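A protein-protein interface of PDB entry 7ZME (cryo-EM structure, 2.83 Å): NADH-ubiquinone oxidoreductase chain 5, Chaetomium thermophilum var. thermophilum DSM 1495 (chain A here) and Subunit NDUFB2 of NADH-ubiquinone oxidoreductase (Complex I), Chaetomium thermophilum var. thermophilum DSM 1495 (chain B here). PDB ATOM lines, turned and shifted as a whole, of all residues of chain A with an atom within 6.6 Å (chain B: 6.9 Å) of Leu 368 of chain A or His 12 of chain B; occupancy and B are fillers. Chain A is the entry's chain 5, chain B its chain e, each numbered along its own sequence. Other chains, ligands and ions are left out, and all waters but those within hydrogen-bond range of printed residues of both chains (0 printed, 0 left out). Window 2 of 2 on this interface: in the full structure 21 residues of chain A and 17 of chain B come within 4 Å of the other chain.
NE2 of His 12 of chain B lies within hydrogen-bond range of O of Gly 466 of chain A, at 3.3 Å.
O of Ala 16 of chain B lies within hydrogen-bond range of OG of Ser 371 of chain A.
Among the printed residues, pairs that only touch across the chains: Pro 367 of chain A with Ala 16 of chain B, Leu 368 of chain A with Ala 16 of chain B, Val 372 of chain A with Leu 19 of chain B, Leu 368 of chain A with Leu 15 of chain B, Val 475 of chain A with Leu 19 of chain B, Leu 368 of chain A with His 12 of chain B and Thr 471 of chain A with His 12 of chain B.
Leu 368 of chain A touches just these residues of chain B: His 12, Leu 15 and Ala 16.
Of chain A, only Leu 368 (3.97 Å), Gly 466 (3.3 Å) and Thr 471 (3.98 Å) come within 4 Å of His 12 of chain B.
Of the printed residues of chain A, Leu 15 of chain B touches Leu 368 (3.9 Å).
Of the printed residues of chain B, Pro 367 of chain A touches Ala 16.
Of the printed residues of chain B, Val 475 of chain A touches Leu 19 (3.95 Å).
Leu 472 of chain A touches none of the printed residues of chain B.
Asp 467 of chain A touches none of the printed residues of chain B.
The nearest residue of chain A that does not touch His 12 of chain B is Glu 465 of chain A (4.4 Å).
The nearest printed residue of chain B that does not touch Pro 367 of chain A is Arg 13 of chain B (4.7 Å).
Of the 10 printed residues of chain B, 4 touch a printed residue of chain A.
Hydrophobic or aromatic side chains of chain B that line the printed part of chain A: His 12, Leu 15, Ala 16 and Leu 19.
Of the 18 printed residues of chain A, 7 touch a printed residue of chain B.
Printed residues of chain A that touch a printed residue of chain B: Pro 367, Leu 368, Ser 371, Val 372, Gly 466, Thr 471 and Val 475.
Among the printed residues, no Asp or Glu carboxylate lies within 4 Å of a Lys or Arg side-chain nitrogen of the other chain.
O of Asp 467 of chain A sits at hydrogen-bond distance from OG1 of Thr 471 of chain A.
The side-chain carboxylate (OE2) of Glu 465 of chain A lies within hydrogen-bond range of the backbone NH (N) of Leu 368 of chain A, at 3.1 Å.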
ATOM      1  N   ILE A 363       6.559 -27.067 -33.422  1.00  0.00           N
ATOM      2  CA  ILE A 363       5.879 -28.032 -32.566  1.00  0.00           C
ATOM      3  C   ILE A 363       6.851 -28.647 -31.568  1.00  0.00           C
ATOM      4  O   ILE A 363       6.516 -28.846 -30.395  1.00  0.00           O
ATOM      5  CB  ILE A 363       5.176 -29.105 -33.416  1.00  0.00           C
ATOM      6  CG1 ILE A 363       4.507 -30.136 -32.506  1.00  0.00           C
ATOM      7  CG2 ILE A 363       6.146 -29.758 -34.382  1.00  0.00           C
ATOM      8  CD1 ILE A 363       3.571 -31.061 -33.219  1.00  0.00           C
ATOM      9  N   TYR A 365       9.318 -27.095 -30.462  1.00  0.00           N
ATOM     10  CA  TYR A 365       9.775 -25.981 -29.648  1.00  0.00           C
ATOM     11  C   TYR A 365       8.697 -25.447 -28.726  1.00  0.00           C
ATOM     12  O   TYR A 365       9.014 -24.858 -27.688  1.00  0.00           O
ATOM     13  CB  TYR A 365      10.270 -24.844 -30.546  1.00  0.00           C
ATOM     14  CG  TYR A 365      11.458 -25.211 -31.399  1.00  0.00           C
ATOM     15  CD1 TYR A 365      11.292 -25.884 -32.599  1.00  0.00           C
ATOM     16  CD2 TYR A 365      12.747 -24.892 -31.002  1.00  0.00           C
ATOM     17  CE1 TYR A 365      12.372 -26.221 -33.381  1.00  0.00           C
ATOM     18  CE2 TYR A 365      13.832 -25.224 -31.777  1.00  0.00           C
ATOM     19  CZ  TYR A 365      13.640 -25.890 -32.967  1.00  0.00           C
ATOM     20  OH  TYR A 365      14.723 -26.226 -33.747  1.00  0.00           O
ATOM     21  N   LEU A 366       7.433 -25.642 -29.086  1.00  0.00           N
ATOM     22  CA  LEU A 366       6.291 -25.186 -28.299  1.00  0.00           C
ATOM     23  C   LEU A 366       5.332 -26.353 -28.122  1.00  0.00           C
ATOM     24  O   LEU A 366       4.247 -26.380 -28.712  1.00  0.00           O
ATOM     25  CB  LEU A 366       5.606 -24.001 -28.978  1.00  0.00           C
ATOM     26  CG  LEU A 366       6.518 -22.826 -29.322  1.00  0.00           C
ATOM     27  CD1 LEU A 366       5.899 -21.953 -30.391  1.00  0.00           C
ATOM     28  CD2 LEU A 366       6.811 -22.021 -28.074  1.00  0.00           C
ATOM     29  N   PRO A 367       5.707 -27.346 -27.309  1.00  0.00           N
ATOM     30  CA  PRO A 367       4.841 -28.527 -27.169  1.00  0.00           C
ATOM     31  C   PRO A 367       3.548 -28.240 -26.430  1.00  0.00           C
ATOM     32  O   PRO A 367       2.486 -28.714 -26.848  1.00  0.00           O
ATOM     33  CB  PRO A 367       5.731 -29.515 -26.408  1.00  0.00           C
ATOM     34  CG  PRO A 367       6.649 -28.654 -25.628  1.00  0.00           C
ATOM     35  CD  PRO A 367       6.918 -27.447 -26.476  1.00  0.00           C
ATOM     36  N   LEU A 368       3.607 -27.488 -25.331  1.00  0.00           N
ATOM     37  CA  LEU A 368       2.384 -27.112 -24.632  1.00  0.00           C
ATOM     38  C   LEU A 368       1.555 -26.137 -25.454  1.00  0.00           C
ATOM     39  O   LEU A 368       0.326 -26.249 -25.505  1.00  0.00           O
ATOM     40  CB  LEU A 368       2.719 -26.511 -23.270  1.00  0.00           C
ATOM     41  CG  LEU A 368       1.511 -26.136 -22.411  1.00  0.00           C
ATOM     42  CD1 LEU A 368       0.692 -27.371 -22.078  1.00  0.00           C
ATOM     43  CD2 LEU A 368       1.958 -25.423 -21.146  1.00  0.00           C
ATOM     44  N   THR A 369       2.211 -25.171 -26.099  1.00  0.00           N
ATOM     45  CA  THR A 369       1.488 -24.193 -26.901  1.00  0.00           C
ATOM     46  C   THR A 369       0.725 -24.866 -28.031  1.00  0.00           C
ATOM     47  O   THR A 369      -0.446 -24.553 -28.272  1.00  0.00           O
ATOM     48  CB  THR A 369       2.456 -23.149 -27.455  1.00  0.00           C
ATOM     49  OG1 THR A 369       3.093 -22.462 -26.374  1.00  0.00           O
ATOM     50  CG2 THR A 369       1.724 -22.147 -28.315  1.00  0.00           C
ATOM     51  N   TYR A 370       1.368 -25.803 -28.731  1.00  0.00           N
ATOM     52  CA  TYR A 370       0.692 -26.493 -29.823  1.00  0.00           C
ATOM     53  C   TYR A 370      -0.489 -27.309 -29.315  1.00  0.00           C
ATOM     54  O   TYR A 370      -1.557 -27.323 -29.937  1.00  0.00           O
ATOM     55  CB  TYR A 370       1.676 -27.388 -30.569  1.00  0.00           C
ATOM     56  CG  TYR A 370       1.005 -28.299 -31.564  1.00  0.00           C
ATOM     57  CD1 TYR A 370       0.534 -27.810 -32.772  1.00  0.00           C
ATOM     58  CD2 TYR A 370       0.826 -29.646 -31.291  1.00  0.00           C
ATOM     59  CE1 TYR A 370      -0.085 -28.633 -33.679  1.00  0.00           C
ATOM     60  CE2 TYR A 370       0.209 -30.476 -32.193  1.00  0.00           C
ATOM     61  CZ  TYR A 370      -0.244 -29.966 -33.386  1.00  0.00           C
ATOM     62  OH  TYR A 370      -0.862 -30.795 -34.286  1.00  0.00           O
ATOM     63  N   SER A 371      -0.312 -28.001 -28.188  1.00  0.00           N
ATOM     64  CA  SER A 371      -1.370 -28.863 -27.675  1.00  0.00           C
ATOM     65  C   SER A 371      -2.608 -28.062 -27.295  1.00  0.00           C
ATOM     66  O   SER A 371      -3.732 -28.461 -27.616  1.00  0.00           O
ATOM     67  CB  SER A 371      -0.854 -29.659 -26.477  1.00  0.00           C
ATOM     68  OG  SER A 371      -1.858 -30.500 -25.943  1.00  0.00           O
ATOM     69  N   VAL A 372      -2.426 -26.926 -26.620  1.00  0.00           N
ATOM     70  CA  VAL A 372      -3.578 -26.129 -26.210  1.00  0.00           C
ATOM     71  C   VAL A 372      -4.223 -25.448 -27.409  1.00  0.00           C
ATOM     72  O   VAL A 372      -5.445 -25.277 -27.446  1.00  0.00           O
ATOM     73  CB  VAL A 372      -3.188 -25.113 -25.117  1.00  0.00           C
ATOM     74  CG1 VAL A 372      -2.570 -25.826 -23.930  1.00  0.00           C
ATOM     75  CG2 VAL A 372      -2.253 -24.048 -25.654  1.00  0.00           C
ATOM     76  N   MET A 373      -3.427 -25.045 -28.402  1.00  0.00           N
ATOM     77  CA  MET A 373      -3.995 -24.441 -29.601  1.00  0.00           C
ATOM     78  C   MET A 373      -4.687 -25.480 -30.471  1.00  0.00           C
ATOM     79  O   MET A 373      -5.599 -25.140 -31.233  1.00  0.00           O
ATOM     80  CB  MET A 373      -2.905 -23.715 -30.386  1.00  0.00           C
ATOM     81  CG  MET A 373      -2.375 -22.473 -29.687  1.00  0.00           C
ATOM     82  SD  MET A 373      -1.520 -21.320 -30.773  1.00  0.00           S
ATOM     83  CE  MET A 373      -2.835 -20.852 -31.887  1.00  0.00           C
ATOM     84  N   GLU A 465       9.519 -22.155 -24.616  1.00  0.00           N
ATOM     85  CA  GLU A 465       8.153 -21.991 -24.153  1.00  0.00           C
ATOM     86  C   GLU A 465       8.090 -20.890 -23.097  1.00  0.00           C
ATOM     87  O   GLU A 465       9.086 -20.233 -22.781  1.00  0.00           O
ATOM     88  CB  GLU A 465       7.608 -23.310 -23.610  1.00  0.00           C
ATOM     89  CG  GLU A 465       6.939 -24.186 -24.660  1.00  0.00           C
ATOM     90  CD  GLU A 465       5.473 -23.848 -24.854  1.00  0.00           C
ATOM     91  OE1 GLU A 465       5.023 -22.811 -24.323  1.00  0.00           O
ATOM     92  OE2 GLU A 465       4.767 -24.619 -25.534  1.00  0.00           O
ATOM     93  N   GLY A 466       6.901 -20.681 -22.544  1.00  0.00           N
ATOM     94  CA  GLY A 466       6.686 -19.627 -21.580  1.00  0.00           C
ATOM     95  C   GLY A 466       7.046 -20.036 -20.165  1.00  0.00           C
ATOM     96  O   GLY A 466       7.600 -21.105 -19.904  1.00  0.00           O
ATOM     97  N   ASP A 467       6.717 -19.147 -19.236  1.00  0.00           N
ATOM     98  CA  ASP A 467       6.927 -19.359 -17.816  1.00  0.00           C
ATOM     99  C   ASP A 467       5.607 -19.750 -17.158  1.00  0.00           C
ATOM    100  O   ASP A 467       4.611 -20.026 -17.829  1.00  0.00           O
ATOM    101  CB  ASP A 467       7.532 -18.107 -17.181  1.00  0.00           C
ATOM    102  CG  ASP A 467       6.542 -16.972 -17.093  1.00  0.00           C
ATOM    103  OD1 ASP A 467       5.777 -16.793 -18.060  1.00  0.00           O
ATOM    104  OD2 ASP A 467       6.525 -16.266 -16.063  1.00  0.00           O
ATOM    105  N   PHE A 468       5.603 -19.790 -15.824  1.00  0.00           N
ATOM    106  CA  PHE A 468       4.418 -20.219 -15.088  1.00  0.00           C
ATOM    107  C   PHE A 468       3.234 -19.298 -15.350  1.00  0.00           C
ATOM    108  O   PHE A 468       2.143 -19.758 -15.707  1.00  0.00           O
ATOM    109  CB  PHE A 468       4.734 -20.282 -13.594  1.00  0.00           C
ATOM    110  CG  PHE A 468       3.517 -20.291 -12.714  1.00  0.00           C
ATOM    111  CD1 PHE A 468       2.731 -21.426 -12.607  1.00  0.00           C
ATOM    112  CD2 PHE A 468       3.163 -19.163 -11.991  1.00  0.00           C
ATOM    113  CE1 PHE A 468       1.612 -21.435 -11.797  1.00  0.00           C
ATOM    114  CE2 PHE A 468       2.046 -19.167 -11.182  1.00  0.00           C
ATOM    115  CZ  PHE A 468       1.270 -20.304 -11.083  1.00  0.00           C
ATOM    116  N   THR A 471       1.801 -19.793 -19.009  1.00  0.00           N
ATOM    117  CA  THR A 471       1.203 -21.060 -19.409  1.00  0.00           C
ATOM    118  C   THR A 471       0.038 -21.482 -18.528  1.00  0.00           C
ATOM    119  O   THR A 471      -0.837 -22.217 -18.996  1.00  0.00           O
ATOM    120  CB  THR A 471       2.258 -22.168 -19.402  1.00  0.00           C
ATOM    121  OG1 THR A 471       2.738 -22.365 -18.066  1.00  0.00           O
ATOM    122  CG2 THR A 471       3.421 -21.798 -20.304  1.00  0.00           C
ATOM    123  N   LEU A 472       0.010 -21.051 -17.268  1.00  0.00           N
ATOM    124  CA  LEU A 472      -1.068 -21.467 -16.371  1.00  0.00           C
ATOM    125  C   LEU A 472      -2.449 -21.104 -16.902  1.00  0.00           C
ATOM    126  O   LEU A 472      -3.346 -21.963 -16.848  1.00  0.00           O
ATOM    127  CB  LEU A 472      -0.837 -20.888 -14.972  1.00  0.00           C
ATOM    128  CG  LEU A 472      -2.013 -21.033 -14.001  1.00  0.00           C
ATOM    129  CD1 LEU A 472      -2.166 -22.477 -13.553  1.00  0.00           C
ATOM    130  CD2 LEU A 472      -1.848 -20.109 -12.806  1.00  0.00           C
ATOM    131  N   LEU A 474      -3.233 -20.942 -19.969  1.00  0.00           N
ATOM    132  CA  LEU A 474      -3.431 -21.805 -21.127  1.00  0.00           C
ATOM    133  C   LEU A 474      -3.903 -23.190 -20.711  1.00  0.00           C
ATOM    134  O   LEU A 474      -4.760 -23.785 -21.375  1.00  0.00           O
ATOM    135  CB  LEU A 474      -2.141 -21.894 -21.938  1.00  0.00           C
ATOM    136  CG  LEU A 474      -1.792 -20.601 -22.673  1.00  0.00           C
ATOM    137  CD1 LEU A 474      -0.511 -20.744 -23.474  1.00  0.00           C
ATOM    138  CD2 LEU A 474      -2.942 -20.190 -23.561  1.00  0.00           C
ATOM    139  N   VAL A 475      -3.359 -23.720 -19.615  1.00  0.00           N
ATOM    140  CA  VAL A 475      -3.797 -25.021 -19.124  1.00  0.00           C
ATOM    141  C   VAL A 475      -5.208 -24.931 -18.561  1.00  0.00           C
ATOM    142  O   VAL A 475      -6.033 -25.825 -18.775  1.00  0.00           O
ATOM    143  CB  VAL A 475      -2.806 -25.562 -18.080  1.00  0.00           C
ATOM    144  CG1 VAL A 475      -3.061 -27.037 -17.822  1.00  0.00           C
ATOM    145  CG2 VAL A 475      -1.380 -25.344 -18.545  1.00  0.00           C
ATOM    146  N   SER B   9      13.503 -27.991 -18.694  1.00  0.00           N
ATOM    147  CA  SER B   9      12.173 -28.056 -18.099  1.00  0.00           C
ATOM    148  C   SER B   9      11.288 -29.053 -18.837  1.00  0.00           C
ATOM    149  O   SER B   9      10.634 -28.708 -19.822  1.00  0.00           O
ATOM    150  CB  SER B   9      11.519 -26.672 -18.098  1.00  0.00           C
ATOM    151  OG  SER B   9      12.268 -25.755 -17.321  1.00  0.00           O
ATOM    152  N   ARG B  10      11.271 -30.294 -18.352  1.00  0.00           N
ATOM    153  CA  ARG B  10      10.446 -31.335 -18.949  1.00  0.00           C
ATOM    154  C   ARG B  10       8.998 -31.285 -18.480  1.00  0.00           C
ATOM    155  O   ARG B  10       8.173 -32.048 -18.995  1.00  0.00           O
ATOM    156  CB  ARG B  10      11.035 -32.714 -18.642  1.00  0.00           C
ATOM    157  N   VAL B  11       8.673 -30.417 -17.519  1.00  0.00           N
ATOM    158  CA  VAL B  11       7.304 -30.331 -17.020  1.00  0.00           C
ATOM    159  C   VAL B  11       6.360 -29.837 -18.107  1.00  0.00           C
ATOM    160  O   VAL B  11       5.182 -30.213 -18.135  1.00  0.00           O
ATOM    161  CB  VAL B  11       7.253 -29.437 -15.763  1.00  0.00           C
ATOM    162  CG1 VAL B  11       7.696 -28.018 -16.090  1.00  0.00           C
ATOM    163  CG2 VAL B  11       5.860 -29.445 -15.151  1.00  0.00           C
ATOM    164  N   HIS B  12       6.853 -28.997 -19.020  1.00  0.00           N
ATOM    165  CA  HIS B  12       6.010 -28.498 -20.100  1.00  0.00           C
ATOM    166  C   HIS B  12       5.545 -29.628 -21.008  1.00  0.00           C
ATOM    167  O   HIS B  12       4.400 -29.628 -21.475  1.00  0.00           O
ATOM    168  CB  HIS B  12       6.758 -27.436 -20.908  1.00  0.00           C
ATOM    169  CG  HIS B  12       6.833 -26.105 -20.231  1.00  0.00           C
ATOM    170  ND1 HIS B  12       8.010 -25.589 -19.733  1.00  0.00           N
ATOM    171  CD2 HIS B  12       5.878 -25.181 -19.972  1.00  0.00           C
ATOM    172  CE1 HIS B  12       7.777 -24.405 -19.196  1.00  0.00           C
ATOM    173  NE2 HIS B  12       6.490 -24.134 -19.328  1.00  0.00           N
ATOM    174  N   ARG B  13       6.423 -30.595 -21.281  1.00  0.00           N
ATOM    175  CA  ARG B  13       6.049 -31.707 -22.150  1.00  0.00           C
ATOM    176  C   ARG B  13       4.937 -32.544 -21.531  1.00  0.00           C
ATOM    177  O   ARG B  13       4.007 -32.967 -22.228  1.00  0.00           O
ATOM    178  CB  ARG B  13       7.272 -32.575 -22.447  1.00  0.00           C
ATOM    179  CG  ARG B  13       7.095 -33.499 -23.639  1.00  0.00           C
ATOM    180  CD  ARG B  13       8.286 -33.425 -24.579  1.00  0.00           C
ATOM    181  NE  ARG B  13       9.502 -33.946 -23.962  1.00  0.00           N
ATOM    182  CZ  ARG B  13      10.714 -33.838 -24.496  1.00  0.00           C
ATOM    183  NH1 ARG B  13      11.766 -34.343 -23.864  1.00  0.00           N
ATOM    184  NH2 ARG B  13      10.877 -33.223 -25.659  1.00  0.00           N
ATOM    185  N   PHE B  14       5.017 -32.800 -20.223  1.00  0.00           N
ATOM    186  CA  PHE B  14       4.002 -33.615 -19.565  1.00  0.00           C
ATOM    187  C   PHE B  14       2.635 -32.944 -19.613  1.00  0.00           C
ATOM    188  O   PHE B  14       1.617 -33.608 -19.836  1.00  0.00           O
ATOM    189  CB  PHE B  14       4.408 -33.900 -18.121  1.00  0.00           C
ATOM    190  CG  PHE B  14       3.330 -34.559 -17.309  1.00  0.00           C
ATOM    191  CD1 PHE B  14       2.974 -35.876 -17.549  1.00  0.00           C
ATOM    192  CD2 PHE B  14       2.671 -33.864 -16.310  1.00  0.00           C
ATOM    193  CE1 PHE B  14       1.982 -36.487 -16.806  1.00  0.00           C
ATOM    194  CE2 PHE B  14       1.679 -34.469 -15.563  1.00  0.00           C
ATOM    195  CZ  PHE B  14       1.333 -35.782 -15.811  1.00  0.00           C
ATOM    196  N   LEU B  15       2.505 -31.715 -19.423  1.00  0.00           N
ATOM    197  CA  LEU B  15       1.183 -31.044 -19.437  1.00  0.00           C
ATOM    198  C   LEU B  15       0.641 -31.073 -20.862  1.00  0.00           C
ATOM    199  O   LEU B  15      -0.566 -31.265 -21.013  1.00  0.00           O
ATOM    200  CB  LEU B  15       1.355 -29.607 -18.938  1.00  0.00           C
ATOM    201  CG  LEU B  15       1.751 -29.466 -17.471  1.00  0.00           C
ATOM    202  CD1 LEU B  15       1.944 -28.003 -17.104  1.00  0.00           C
ATOM    203  CD2 LEU B  15       0.709 -30.109 -16.571  1.00  0.00           C
ATOM    204  N   ALA B  16       1.577 -30.828 -21.875  1.00  0.00           N
ATOM    205  CA  ALA B  16       1.105 -30.908 -23.254  1.00  0.00           C
ATOM    206  C   ALA B  16       0.486 -32.266 -23.545  1.00  0.00           C
ATOM    207  O   ALA B  16      -0.641 -32.355 -24.044  1.00  0.00           O
ATOM    208  CB  ALA B  16       2.261 -30.640 -24.214  1.00  0.00           C
ATOM    209  N   THR B  17       1.217 -33.339 -23.239  1.00  0.00           N
ATOM    210  CA  THR B  17       0.705 -34.679 -23.498  1.00  0.00           C
ATOM    211  C   THR B  17      -0.537 -34.960 -22.663  1.00  0.00           C
ATOM    212  O   THR B  17      -1.505 -35.549 -23.157  1.00  0.00           O
ATOM    213  CB  THR B  17       1.792 -35.716 -23.216  1.00  0.00           C
ATOM    214  OG1 THR B  17       2.917 -35.470 -24.070  1.00  0.00           O
ATOM    215  CG2 THR B  17       1.271 -37.117 -23.481  1.00  0.00           C
ATOM    216  N   LEU B  19      -2.874 -32.912 -21.527  1.00  0.00           N
ATOM    217  CA  LEU B  19      -4.046 -32.263 -22.103  1.00  0.00           C
ATOM    218  C   LEU B  19      -4.489 -32.962 -23.379  1.00  0.00           C
ATOM    219  O   LEU B  19      -5.687 -33.164 -23.602  1.00  0.00           O
ATOM    220  CB  LEU B  19      -3.749 -30.792 -22.369  1.00  0.00           C
ATOM    221  CG  LEU B  19      -3.531 -29.953 -21.116  1.00  0.00           C
ATOM    222  CD1 LEU B  19      -3.151 -28.529 -21.480  1.00  0.00           C
ATOM    223  CD2 LEU B  19      -4.780 -29.974 -20.260  1.00  0.00           C
